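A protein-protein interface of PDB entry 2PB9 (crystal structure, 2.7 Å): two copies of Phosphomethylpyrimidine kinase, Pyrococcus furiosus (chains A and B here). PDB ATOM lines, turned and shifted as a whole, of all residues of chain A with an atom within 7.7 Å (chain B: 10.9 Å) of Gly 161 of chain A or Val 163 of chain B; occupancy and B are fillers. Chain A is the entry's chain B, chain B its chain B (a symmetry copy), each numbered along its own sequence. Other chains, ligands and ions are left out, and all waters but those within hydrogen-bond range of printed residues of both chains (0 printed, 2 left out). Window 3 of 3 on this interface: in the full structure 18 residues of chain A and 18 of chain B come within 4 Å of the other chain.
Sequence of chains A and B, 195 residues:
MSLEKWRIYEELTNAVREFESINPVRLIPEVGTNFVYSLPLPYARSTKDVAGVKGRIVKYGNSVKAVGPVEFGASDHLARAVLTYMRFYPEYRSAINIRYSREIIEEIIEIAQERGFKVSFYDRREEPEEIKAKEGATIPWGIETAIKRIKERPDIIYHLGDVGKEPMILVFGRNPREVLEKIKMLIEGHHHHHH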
ATOM      1  N   TYR A 100      17.141 -12.381  22.786  1.00  0.00           N
ATOM      2  CA  TYR A 100      16.792 -12.049  24.160  1.00  0.00           C
ATOM      3  C   TYR A 100      17.359 -13.090  25.121  1.00  0.00           C
ATOM      4  O   TYR A 100      17.538 -14.251  24.755  1.00  0.00           O
ATOM      5  CB  TYR A 100      15.277 -12.014  24.347  1.00  0.00           C
ATOM      6  CG  TYR A 100      14.898 -11.893  25.802  1.00  0.00           C
ATOM      7  CD1 TYR A 100      14.929 -10.654  26.447  1.00  0.00           C
ATOM      8  CD2 TYR A 100      14.606 -13.027  26.570  1.00  0.00           C
ATOM      9  CE1 TYR A 100      14.684 -10.543  27.815  1.00  0.00           C
ATOM     10  CE2 TYR A 100      14.363 -12.931  27.945  1.00  0.00           C
ATOM     11  CZ  TYR A 100      14.404 -11.683  28.562  1.00  0.00           C
ATOM     12  OH  TYR A 100      14.178 -11.556  29.923  1.00  0.00           O
ATOM     13  N   ASP A 123       3.650  -7.247  26.521  1.00  0.00           N
ATOM     14  CA  ASP A 123       3.429  -8.653  26.827  1.00  0.00           C
ATOM     15  C   ASP A 123       2.211  -9.208  26.102  1.00  0.00           C
ATOM     16  O   ASP A 123       1.077  -8.785  26.348  1.00  0.00           O
ATOM     17  CB  ASP A 123       3.256  -8.827  28.341  1.00  0.00           C
ATOM     18  CG  ASP A 123       3.331 -10.281  28.781  1.00  0.00           C
ATOM     19  OD1 ASP A 123       3.074 -11.185  27.948  1.00  0.00           O
ATOM     20  OD2 ASP A 123       3.643 -10.514  29.969  1.00  0.00           O
ATOM     21  N   ARG A 124       2.457 -10.169  25.220  1.00  0.00           N
ATOM     22  CA  ARG A 124       1.395 -10.778  24.438  1.00  0.00           C
ATOM     23  C   ARG A 124       0.342 -11.438  25.314  1.00  0.00           C
ATOM     24  O   ARG A 124      -0.724 -11.806  24.835  1.00  0.00           O
ATOM     25  CB  ARG A 124       1.987 -11.786  23.447  1.00  0.00           C
ATOM     26  CG  ARG A 124       3.009 -11.148  22.521  1.00  0.00           C
ATOM     27  CD  ARG A 124       3.463 -12.053  21.384  1.00  0.00           C
ATOM     28  NE  ARG A 124       4.395 -11.347  20.503  1.00  0.00           N
ATOM     29  CZ  ARG A 124       4.753 -11.763  19.290  1.00  0.00           C
ATOM     30  NH1 ARG A 124       4.257 -12.896  18.804  1.00  0.00           N
ATOM     31  NH2 ARG A 124       5.592 -11.034  18.553  1.00  0.00           N
ATOM     32  N   ARG A 125       0.638 -11.591  26.600  1.00  0.00           N
ATOM     33  CA  ARG A 125      -0.331 -12.183  27.513  1.00  0.00           C
ATOM     34  C   ARG A 125      -1.373 -11.136  27.891  1.00  0.00           C
ATOM     35  O   ARG A 125      -2.526 -11.471  28.129  1.00  0.00           O
ATOM     36  CB  ARG A 125       0.346 -12.716  28.787  1.00  0.00           C
ATOM     37  CG  ARG A 125       0.900 -14.126  28.666  1.00  0.00           C
ATOM     38  CD  ARG A 125       1.417 -14.643  29.996  1.00  0.00           C
ATOM     39  NE  ARG A 125       2.431 -13.763  30.557  1.00  0.00           N
ATOM     40  CZ  ARG A 125       3.217 -14.075  31.585  1.00  0.00           C
ATOM     41  NH1 ARG A 125       3.114 -15.259  32.180  1.00  0.00           N
ATOM     42  NH2 ARG A 125       4.119 -13.199  32.015  1.00  0.00           N
ATOM     43  N   TYR A 158      11.328  -4.565  24.344  1.00  0.00           N
ATOM     44  CA  TYR A 158      11.484  -6.007  24.305  1.00  0.00           C
ATOM     45  C   TYR A 158      10.175  -6.703  24.655  1.00  0.00           C
ATOM     46  O   TYR A 158       9.151  -6.055  24.855  1.00  0.00           O
ATOM     47  CB  TYR A 158      12.608  -6.437  25.262  1.00  0.00           C
ATOM     48  CG  TYR A 158      12.231  -6.466  26.727  1.00  0.00           C
ATOM     49  CD1 TYR A 158      11.704  -7.620  27.310  1.00  0.00           C
ATOM     50  CD2 TYR A 158      12.397  -5.339  27.533  1.00  0.00           C
ATOM     51  CE1 TYR A 158      11.352  -7.652  28.658  1.00  0.00           C
ATOM     52  CE2 TYR A 158      12.047  -5.358  28.883  1.00  0.00           C
ATOM     53  CZ  TYR A 158      11.524  -6.518  29.439  1.00  0.00           C
ATOM     54  OH  TYR A 158      11.159  -6.538  30.768  1.00  0.00           O
ATOM     55  N   HIS A 159      10.212  -8.027  24.684  1.00  0.00           N
ATOM     56  CA  HIS A 159       9.056  -8.837  25.038  1.00  0.00           C
ATOM     57  C   HIS A 159       9.539 -10.264  25.225  1.00  0.00           C
ATOM     58  O   HIS A 159      10.446 -10.723  24.529  1.00  0.00           O
ATOM     59  CB  HIS A 159       7.972  -8.769  23.958  1.00  0.00           C
ATOM     60  CG  HIS A 159       8.322  -9.476  22.686  1.00  0.00           C
ATOM     61  ND1 HIS A 159       8.159 -10.835  22.519  1.00  0.00           N
ATOM     62  CD2 HIS A 159       8.785  -9.007  21.501  1.00  0.00           C
ATOM     63  CE1 HIS A 159       8.501 -11.171  21.287  1.00  0.00           C
ATOM     64  NE2 HIS A 159       8.883 -10.079  20.649  1.00  0.00           N
ATOM     65  N   LEU A 160       8.943 -10.957  26.184  1.00  0.00           N
ATOM     66  CA  LEU A 160       9.328 -12.328  26.470  1.00  0.00           C
ATOM     67  C   LEU A 160       8.696 -13.311  25.488  1.00  0.00           C
ATOM     68  O   LEU A 160       7.965 -12.919  24.574  1.00  0.00           O
ATOM     69  CB  LEU A 160       8.924 -12.682  27.896  1.00  0.00           C
ATOM     70  CG  LEU A 160       9.430 -11.706  28.950  1.00  0.00           C
ATOM     71  CD1 LEU A 160       8.695 -11.970  30.241  1.00  0.00           C
ATOM     72  CD2 LEU A 160      10.934 -11.841  29.126  1.00  0.00           C
ATOM     73  N   GLY A 161       8.981 -14.591  25.684  1.00  0.00           N
ATOM     74  CA  GLY A 161       8.433 -15.593  24.798  1.00  0.00           C
ATOM     75  C   GLY A 161       6.955 -15.865  25.004  1.00  0.00           C
ATOM     76  O   GLY A 161       6.396 -15.650  26.081  1.00  0.00           O
ATOM     77  N   ASP A 162       6.321 -16.346  23.947  1.00  0.00           N
ATOM     78  CA  ASP A 162       4.908 -16.679  23.980  1.00  0.00           C
ATOM     79  C   ASP A 162       4.802 -18.030  23.296  1.00  0.00           C
ATOM     80  O   ASP A 162       5.751 -18.466  22.644  1.00  0.00           O
ATOM     81  CB  ASP A 162       4.120 -15.604  23.242  1.00  0.00           C
ATOM     82  CG  ASP A 162       4.254 -14.234  23.908  1.00  0.00           C
ATOM     83  OD1 ASP A 162       3.576 -14.014  24.945  1.00  0.00           O
ATOM     84  OD2 ASP A 162       5.048 -13.395  23.403  1.00  0.00           O
ATOM     85  N   VAL A 163       3.676 -18.714  23.446  1.00  0.00           N
ATOM     86  CA  VAL A 163       3.566 -20.024  22.820  1.00  0.00           C
ATOM     87  C   VAL A 163       3.884 -19.937  21.318  1.00  0.00           C
ATOM     88  O   VAL A 163       3.260 -19.181  20.579  1.00  0.00           O
ATOM     89  CB  VAL A 163       2.167 -20.638  23.070  1.00  0.00           C
ATOM     90  CG1 VAL A 163       2.056 -22.008  22.426  1.00  0.00           C
ATOM     91  CG2 VAL A 163       1.940 -20.770  24.558  1.00  0.00           C
ATOM     92  N   GLY A 164       4.893 -20.683  20.884  1.00  0.00           N
ATOM     93  CA  GLY A 164       5.263 -20.671  19.484  1.00  0.00           C
ATOM     94  C   GLY A 164       6.088 -19.479  19.049  1.00  0.00           C
ATOM     95  O   GLY A 164       6.614 -19.472  17.942  1.00  0.00           O
ATOM     96  N   LYS A 165       6.208 -18.465  19.902  1.00  0.00           N
ATOM     97  CA  LYS A 165       6.984 -17.268  19.559  1.00  0.00           C
ATOM     98  C   LYS A 165       8.092 -16.998  20.572  1.00  0.00           C
ATOM     99  O   LYS A 165       7.867 -17.009  21.776  1.00  0.00           O
ATOM    100  CB  LYS A 165       6.082 -16.024  19.487  1.00  0.00           C
ATOM    101  CG  LYS A 165       4.885 -16.131  18.552  1.00  0.00           C
ATOM    102  CD  LYS A 165       3.591 -16.098  19.354  1.00  0.00           C
ATOM    103  CE  LYS A 165       2.337 -16.192  18.469  1.00  0.00           C
ATOM    104  NZ  LYS A 165       2.085 -14.959  17.661  1.00  0.00           N
ATOM    105  N   GLU A 166       9.287 -16.723  20.071  1.00  0.00           N
ATOM    106  CA  GLU A 166      10.429 -16.450  20.930  1.00  0.00           C
ATOM    107  C   GLU A 166      10.480 -15.013  21.449  1.00  0.00           C
ATOM    108  O   GLU A 166       9.832 -14.111  20.917  1.00  0.00           O
ATOM    109  CB  GLU A 166      11.726 -16.745  20.171  1.00  0.00           C
ATOM    110  CG  GLU A 166      11.525 -17.408  18.827  1.00  0.00           C
ATOM    111  CD  GLU A 166      12.823 -17.977  18.261  1.00  0.00           C
ATOM    112  OE1 GLU A 166      13.788 -17.195  18.019  1.00  0.00           O
ATOM    113  OE2 GLU A 166      12.865 -19.219  18.066  1.00  0.00           O
ATOM    114  N   PRO A 167      11.248 -14.788  22.520  1.00  0.00           N
ATOM    115  CA  PRO A 167      11.349 -13.430  23.055  1.00  0.00           C
ATOM    116  C   PRO A 167      12.202 -12.620  22.078  1.00  0.00           C
ATOM    117  O   PRO A 167      12.908 -13.195  21.260  1.00  0.00           O
ATOM    118  CB  PRO A 167      12.047 -13.646  24.396  1.00  0.00           C
ATOM    119  CG  PRO A 167      12.931 -14.825  24.116  1.00  0.00           C
ATOM    120  CD  PRO A 167      12.012 -15.741  23.344  1.00  0.00           C
ATOM    121  N   MET A 168      12.144 -11.300  22.155  1.00  0.00           N
ATOM    122  CA  MET A 168      12.938 -10.477  21.264  1.00  0.00           C
ATOM    123  C   MET A 168      13.221  -9.123  21.872  1.00  0.00           C
ATOM    124  O   MET A 168      12.426  -8.597  22.656  1.00  0.00           O
ATOM    125  CB  MET A 168      12.223 -10.275  19.925  1.00  0.00           C
ATOM    126  CG  MET A 168      12.511 -11.337  18.868  1.00  0.00           C
ATOM    127  SD  MET A 168      14.378 -11.356  18.342  1.00  0.00           S
ATOM    128  CE  MET A 168      14.674  -9.452  18.465  1.00  0.00           C
ATOM    129  N   ASP B 123       5.157 -33.859  23.269  1.00  0.00           N
ATOM    130  CA  ASP B 123       4.663 -32.595  23.797  1.00  0.00           C
ATOM    131  C   ASP B 123       5.480 -32.121  24.991  1.00  0.00           C
ATOM    132  O   ASP B 123       5.501 -32.765  26.043  1.00  0.00           O
ATOM    133  CB  ASP B 123       3.192 -32.748  24.203  1.00  0.00           C
ATOM    134  CG  ASP B 123       2.510 -31.416  24.470  1.00  0.00           C
ATOM    135  OD1 ASP B 123       3.213 -30.423  24.783  1.00  0.00           O
ATOM    136  OD2 ASP B 123       1.265 -31.369  24.372  1.00  0.00           O
ATOM    137  N   ARG B 124       6.136 -30.979  24.818  1.00  0.00           N
ATOM    138  CA  ARG B 124       6.973 -30.415  25.863  1.00  0.00           C
ATOM    139  C   ARG B 124       6.188 -30.121  27.132  1.00  0.00           C
ATOM    140  O   ARG B 124       6.773 -29.850  28.175  1.00  0.00           O
ATOM    141  CB  ARG B 124       7.670 -29.150  25.350  1.00  0.00           C
ATOM    142  CG  ARG B 124       8.504 -29.418  24.108  1.00  0.00           C
ATOM    143  CD  ARG B 124       9.382 -28.248  23.690  1.00  0.00           C
ATOM    144  NE  ARG B 124      10.199 -28.605  22.528  1.00  0.00           N
ATOM    145  CZ  ARG B 124      11.250 -27.908  22.098  1.00  0.00           C
ATOM    146  NH1 ARG B 124      11.617 -26.801  22.734  1.00  0.00           N
ATOM    147  NH2 ARG B 124      11.946 -28.332  21.043  1.00  0.00           N
ATOM    148  N   ARG B 125       4.864 -30.174  27.047  1.00  0.00           N
ATOM    149  CA  ARG B 125       4.041 -29.939  28.226  1.00  0.00           C
ATOM    150  C   ARG B 125       4.023 -31.197  29.087  1.00  0.00           C
ATOM    151  O   ARG B 125       3.929 -31.111  30.304  1.00  0.00           O
ATOM    152  CB  ARG B 125       2.602 -29.558  27.843  1.00  0.00           C
ATOM    153  CG  ARG B 125       2.392 -28.078  27.562  1.00  0.00           C
ATOM    154  CD  ARG B 125       0.927 -27.751  27.339  1.00  0.00           C
ATOM    155  NE  ARG B 125       0.358 -28.542  26.259  1.00  0.00           N
ATOM    156  CZ  ARG B 125      -0.825 -28.309  25.693  1.00  0.00           C
ATOM    157  NH1 ARG B 125      -1.582 -27.297  26.103  1.00  0.00           N
ATOM    158  NH2 ARG B 125      -1.248 -29.090  24.705  1.00  0.00           N
ATOM    159  N   GLU B 127       6.460 -33.054  29.384  1.00  0.00           N
ATOM    160  CA  GLU B 127       7.868 -33.249  29.714  1.00  0.00           C
ATOM    161  C   GLU B 127       8.118 -32.937  31.189  1.00  0.00           C
ATOM    162  O   GLU B 127       7.833 -31.832  31.657  1.00  0.00           O
ATOM    163  CB  GLU B 127       8.744 -32.329  28.850  1.00  0.00           C
ATOM    164  CG  GLU B 127      10.250 -32.560  28.958  1.00  0.00           C
ATOM    165  CD  GLU B 127      11.051 -31.636  28.036  1.00  0.00           C
ATOM    166  OE1 GLU B 127      10.512 -31.220  26.987  1.00  0.00           O
ATOM    167  OE2 GLU B 127      12.228 -31.326  28.338  1.00  0.00           O
ATOM    168  N   GLU B 129       9.588 -31.665  34.525  1.00  0.00           N
ATOM    169  CA  GLU B 129      10.380 -30.481  34.812  1.00  0.00           C
ATOM    170  C   GLU B 129      11.865 -30.820  34.949  1.00  0.00           C
ATOM    171  O   GLU B 129      12.726 -30.063  34.502  1.00  0.00           O
ATOM    172  CB  GLU B 129       9.855 -29.830  36.096  1.00  0.00           C
ATOM    173  CG  GLU B 129      10.290 -28.400  36.279  1.00  0.00           C
ATOM    174  CD  GLU B 129       9.945 -27.543  35.075  1.00  0.00           C
ATOM    175  OE1 GLU B 129       8.755 -27.509  34.678  1.00  0.00           O
ATOM    176  OE2 GLU B 129      10.872 -26.907  34.533  1.00  0.00           O
ATOM    177  N   LYS B 132      13.558 -30.807  31.654  1.00  0.00           N
ATOM    178  CA  LYS B 132      13.636 -29.475  31.053  1.00  0.00           C
ATOM    179  C   LYS B 132      14.812 -28.702  31.643  1.00  0.00           C
ATOM    180  O   LYS B 132      15.323 -27.746  31.038  1.00  0.00           O
ATOM    181  CB  LYS B 132      12.345 -28.689  31.294  1.00  0.00           C
ATOM    182  CG  LYS B 132      11.106 -29.262  30.617  1.00  0.00           C
ATOM    183  CD  LYS B 132       9.894 -28.376  30.865  1.00  0.00           C
ATOM    184  CE  LYS B 132       8.658 -28.942  30.202  1.00  0.00           C
ATOM    185  NZ  LYS B 132       7.432 -28.171  30.545  1.00  0.00           N
ATOM    186  N   THR B 138      16.188 -32.261  26.029  1.00  0.00           N
ATOM    187  CA  THR B 138      14.829 -32.222  25.540  1.00  0.00           C
ATOM    188  C   THR B 138      14.664 -32.886  24.186  1.00  0.00           C
ATOM    189  O   THR B 138      13.733 -33.662  23.990  1.00  0.00           O
ATOM    190  CB  THR B 138      14.332 -30.769  25.473  1.00  0.00           C
ATOM    191  OG1 THR B 138      14.147 -30.276  26.806  1.00  0.00           O
ATOM    192  CG2 THR B 138      13.034 -30.678  24.711  1.00  0.00           C
ATOM    193  N   HIS B 159       5.713 -31.660  16.795  1.00  0.00           N
ATOM    194  CA  HIS B 159       5.428 -31.137  18.123  1.00  0.00           C
ATOM    195  C   HIS B 159       4.928 -29.714  17.956  1.00  0.00           C
ATOM    196  O   HIS B 159       5.377 -28.984  17.069  1.00  0.00           O
ATOM    197  CB  HIS B 159       6.671 -31.174  19.018  1.00  0.00           C
ATOM    198  CG  HIS B 159       7.731 -30.185  18.644  1.00  0.00           C
ATOM    199  ND1 HIS B 159       7.694 -28.866  19.043  1.00  0.00           N
ATOM    200  CD2 HIS B 159       8.882 -30.333  17.944  1.00  0.00           C
ATOM    201  CE1 HIS B 159       8.778 -28.246  18.610  1.00  0.00           C
ATOM    202  NE2 HIS B 159       9.516 -29.115  17.941  1.00  0.00           N
ATOM    203  N   LEU B 160       3.981 -29.328  18.798  1.00  0.00           N
ATOM    204  CA  LEU B 160       3.411 -27.994  18.728  1.00  0.00           C
ATOM    205  C   LEU B 160       4.308 -26.958  19.401  1.00  0.00           C
ATOM    206  O   LEU B 160       5.385 -27.281  19.912  1.00  0.00           O
ATOM    207  CB  LEU B 160       2.034 -27.994  19.381  1.00  0.00           C
ATOM    208  CG  LEU B 160       1.088 -29.059  18.842  1.00  0.00           C
ATOM    209  CD1 LEU B 160      -0.088 -29.176  19.782  1.00  0.00           C
ATOM    210  CD2 LEU B 160       0.642 -28.713  17.431  1.00  0.00           C
ATOM    211  N   GLY B 161       3.858 -25.711  19.398  1.00  0.00           N
ATOM    212  CA  GLY B 161       4.645 -24.662  20.005  1.00  0.00           C
ATOM    213  C   GLY B 161       4.647 -24.684  21.521  1.00  0.00           C
ATOM    214  O   GLY B 161       3.730 -25.192  22.168  1.00  0.00           O
ATOM    215  N   ASP B 162       5.701 -24.119  22.089  1.00  0.00           N
ATOM    216  CA  ASP B 162       5.851 -24.038  23.531  1.00  0.00           C
ATOM    217  C   ASP B 162       6.309 -22.616  23.804  1.00  0.00           C
ATOM    218  O   ASP B 162       6.711 -21.911  22.878  1.00  0.00           O
ATOM    219  CB  ASP B 162       6.878 -25.065  23.989  1.00  0.00           C
ATOM    220  CG  ASP B 162       6.436 -26.496  23.684  1.00  0.00           C
ATOM    221  OD1 ASP B 162       5.578 -27.023  24.439  1.00  0.00           O
ATOM    222  OD2 ASP B 162       6.933 -27.078  22.681  1.00  0.00           O
ATOM    223  N   VAL B 163       6.239 -22.170  25.050  1.00  0.00           N
ATOM    224  CA  VAL B 163       6.648 -20.801  25.326  1.00  0.00           C
ATOM    225  C   VAL B 163       8.068 -20.542  24.799  1.00  0.00           C
ATOM    226  O   VAL B 163       9.017 -21.233  25.159  1.00  0.00           O
ATOM    227  CB  VAL B 163       6.538 -20.488  26.839  1.00  0.00           C
ATOM    228  CG1 VAL B 163       6.954 -19.057  27.125  1.00  0.00           C
ATOM    229  CG2 VAL B 163       5.107 -20.687  27.286  1.00  0.00           C
ATOM    230  N   GLY B 164       8.197 -19.569  23.904  1.00  0.00           N
ATOM    231  CA  GLY B 164       9.498 -19.248  23.354  1.00  0.00           C
ATOM    232  C   GLY B 164       9.980 -20.179  22.263  1.00  0.00           C
ATOM    233  O   GLY B 164      10.968 -19.884  21.601  1.00  0.00           O
ATOM    234  N   LYS B 165       9.299 -21.305  22.065  1.00  0.00           N
ATOM    235  CA  LYS B 165       9.701 -22.267  21.032  1.00  0.00           C
ATOM    236  C   LYS B 165       8.576 -22.541  20.040  1.00  0.00           C
ATOM    237  O   LYS B 165       7.441 -22.801  20.423  1.00  0.00           O
ATOM    238  CB  LYS B 165      10.128 -23.606  21.659  1.00  0.00           C
ATOM    239  CG  LYS B 165      11.220 -23.520  22.716  1.00  0.00           C
ATOM    240  CD  LYS B 165      10.663 -23.921  24.075  1.00  0.00           C
ATOM    241  CE  LYS B 165      11.718 -23.867  25.193  1.00  0.00           C
ATOM    242  NZ  LYS B 165      12.750 -24.945  25.091  1.00  0.00           N
ATOM    243  N   GLU B 166       8.907 -22.512  18.758  1.00  0.00           N
ATOM    244  CA  GLU B 166       7.927 -22.752  17.711  1.00  0.00           C
ATOM    245  C   GLU B 166       7.652 -24.234  17.453  1.00  0.00           C
ATOM    246  O   GLU B 166       8.427 -25.111  17.836  1.00  0.00           O
ATOM    247  CB  GLU B 166       8.397 -22.105  16.406  1.00  0.00           C
ATOM    248  CG  GLU B 166       9.627 -21.237  16.548  1.00  0.00           C
ATOM    249  CD  GLU B 166       9.865 -20.362  15.321  1.00  0.00           C
ATOM    250  OE1 GLU B 166      10.069 -20.911  14.199  1.00  0.00           O
ATOM    251  OE2 GLU B 166       9.842 -19.116  15.494  1.00  0.00           O
ATOM    252  N   PRO B 167       6.520 -24.532  16.807  1.00  0.00           N
ATOM    253  CA  PRO B 167       6.208 -25.931  16.518  1.00  0.00           C
ATOM    254  C   PRO B 167       7.149 -26.384  15.400  1.00  0.00           C
ATOM    255  O   PRO B 167       7.730 -25.553  14.716  1.00  0.00           O
ATOM    256  CB  PRO B 167       4.752 -25.866  16.062  1.00  0.00           C
ATOM    257  CG  PRO B 167       4.680 -24.526  15.394  1.00  0.00           C
ATOM    258  CD  PRO B 167       5.433 -23.643  16.360  1.00  0.00           C
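The backbone NH of Gly 164 of chain B is in hydrogen-bond range of the backbone carbonyl oxygen of Asp 162 of chain A, at 3.0 Å. The backbone NH (N) of Gly 164 of chain A lies within hydrogen-bond range of the backbone carbonyl oxygen (O) of Asp 162 of chain B (3.0 Å). The backbone carbonyl oxygen (O) of Lys 165 of chain B lies close to the backbone NH (N) of Gly 164 of chain A. O of Lys 165 of chain A sits close to N of Gly 164 of chain B (3.3 Å).
The side-chain carboxylate of Asp 162 of chain A lies within salt-bridge range of the guanidinium group of Arg 124 of chain A (3.6 Å). The side-chain carboxylate of Asp 162 of chain B is in salt-bridge range of the guanidinium group of Arg 124 of chain B (3.6 Å).
Among the printed residues, pairs that only touch across the chains: Gly 164 of chain A with Glu 166 of chain B (3.5 Å), Glu 166 of chain A with Gly 164 of chain B (3.5 Å), Asp 162 of chain A with Asp 162 of chain B (3.6 Å), Val 163 of chain A with Gly 161 of chain B (3.6 Å), Gly 161 of chain A with Val 163 of chain B (3.6 Å), Asp 162 of chain A with Val 163 of chain B (3.7 Å), Val 163 of chain A with Asp 162 of chain B (3.7 Å) and Glu 166 of chain A with Glu 166 of chain B (3.97 Å).
Gly 161 of chain A touches one residue of chain B. Of the printed residues of chain A, Val 163 of chain B touches Gly 161 and Asp 162. No residue of chain B comes within 4 Å of Leu 160 of chain A. Asp 162 of chain A touches just these residues of chain B: Asp 162, Val 163 and Gly 164. No residue of chain B comes within 4 Å of Pro 167 of chain A. Printed residues of chain B within 4 Å of Lys 165 of chain A: Gly 164 (3.2 Å). Of the printed residues of chain B, Gly 164 of chain A touches Asp 162 (3.0 Å), Lys 165 (3.2 Å) and Glu 166 (3.5 Å). Of the printed residues of chain A, Gly 161 of chain B touches Val 163 (3.6 Å). Of the printed residues of chain A, Asp 162 of chain B touches Asp 162, Val 163 and Gly 164. Of the printed residues of chain A, Glu 166 of chain B touches Gly 164 and Glu 166. Thr 138 of chain B touches none of the printed residues of chain A. The nearest residue of chain A that does not touch Val 163 of chain B is Val 163 of chain A (4.05 Å).
Of the 16 printed residues of chain B, 6 touch a printed residue of chain A. Hydrophobic or aromatic side chains of chain B within 4 Å of the printed part of chain A: Val 163. Hydrophobic or aromatic side chains of chain A that line the printed part of chain B: Val 163.
Gly 161 of chain A touches Val 163 of chain B, and with the chains exchanged Val 163 of chain A touches Gly 161 of chain B. Asp 162 of chain A touches Val 163 of chain B, and with the chains exchanged Val 163 of chain A touches Asp 162 of chain B. Asp 162 of chain A touches Gly 164 of chain B, and with the chains exchanged Gly 164 of chain A touches Asp 162 of chain B. Glu 166 of chain A touches its own counterpart, Glu 166 of chain B. Positions printed for both chains: 123, 124, 125, 159, 160, 161, 162, 163, 164, 165, 166 and 167.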
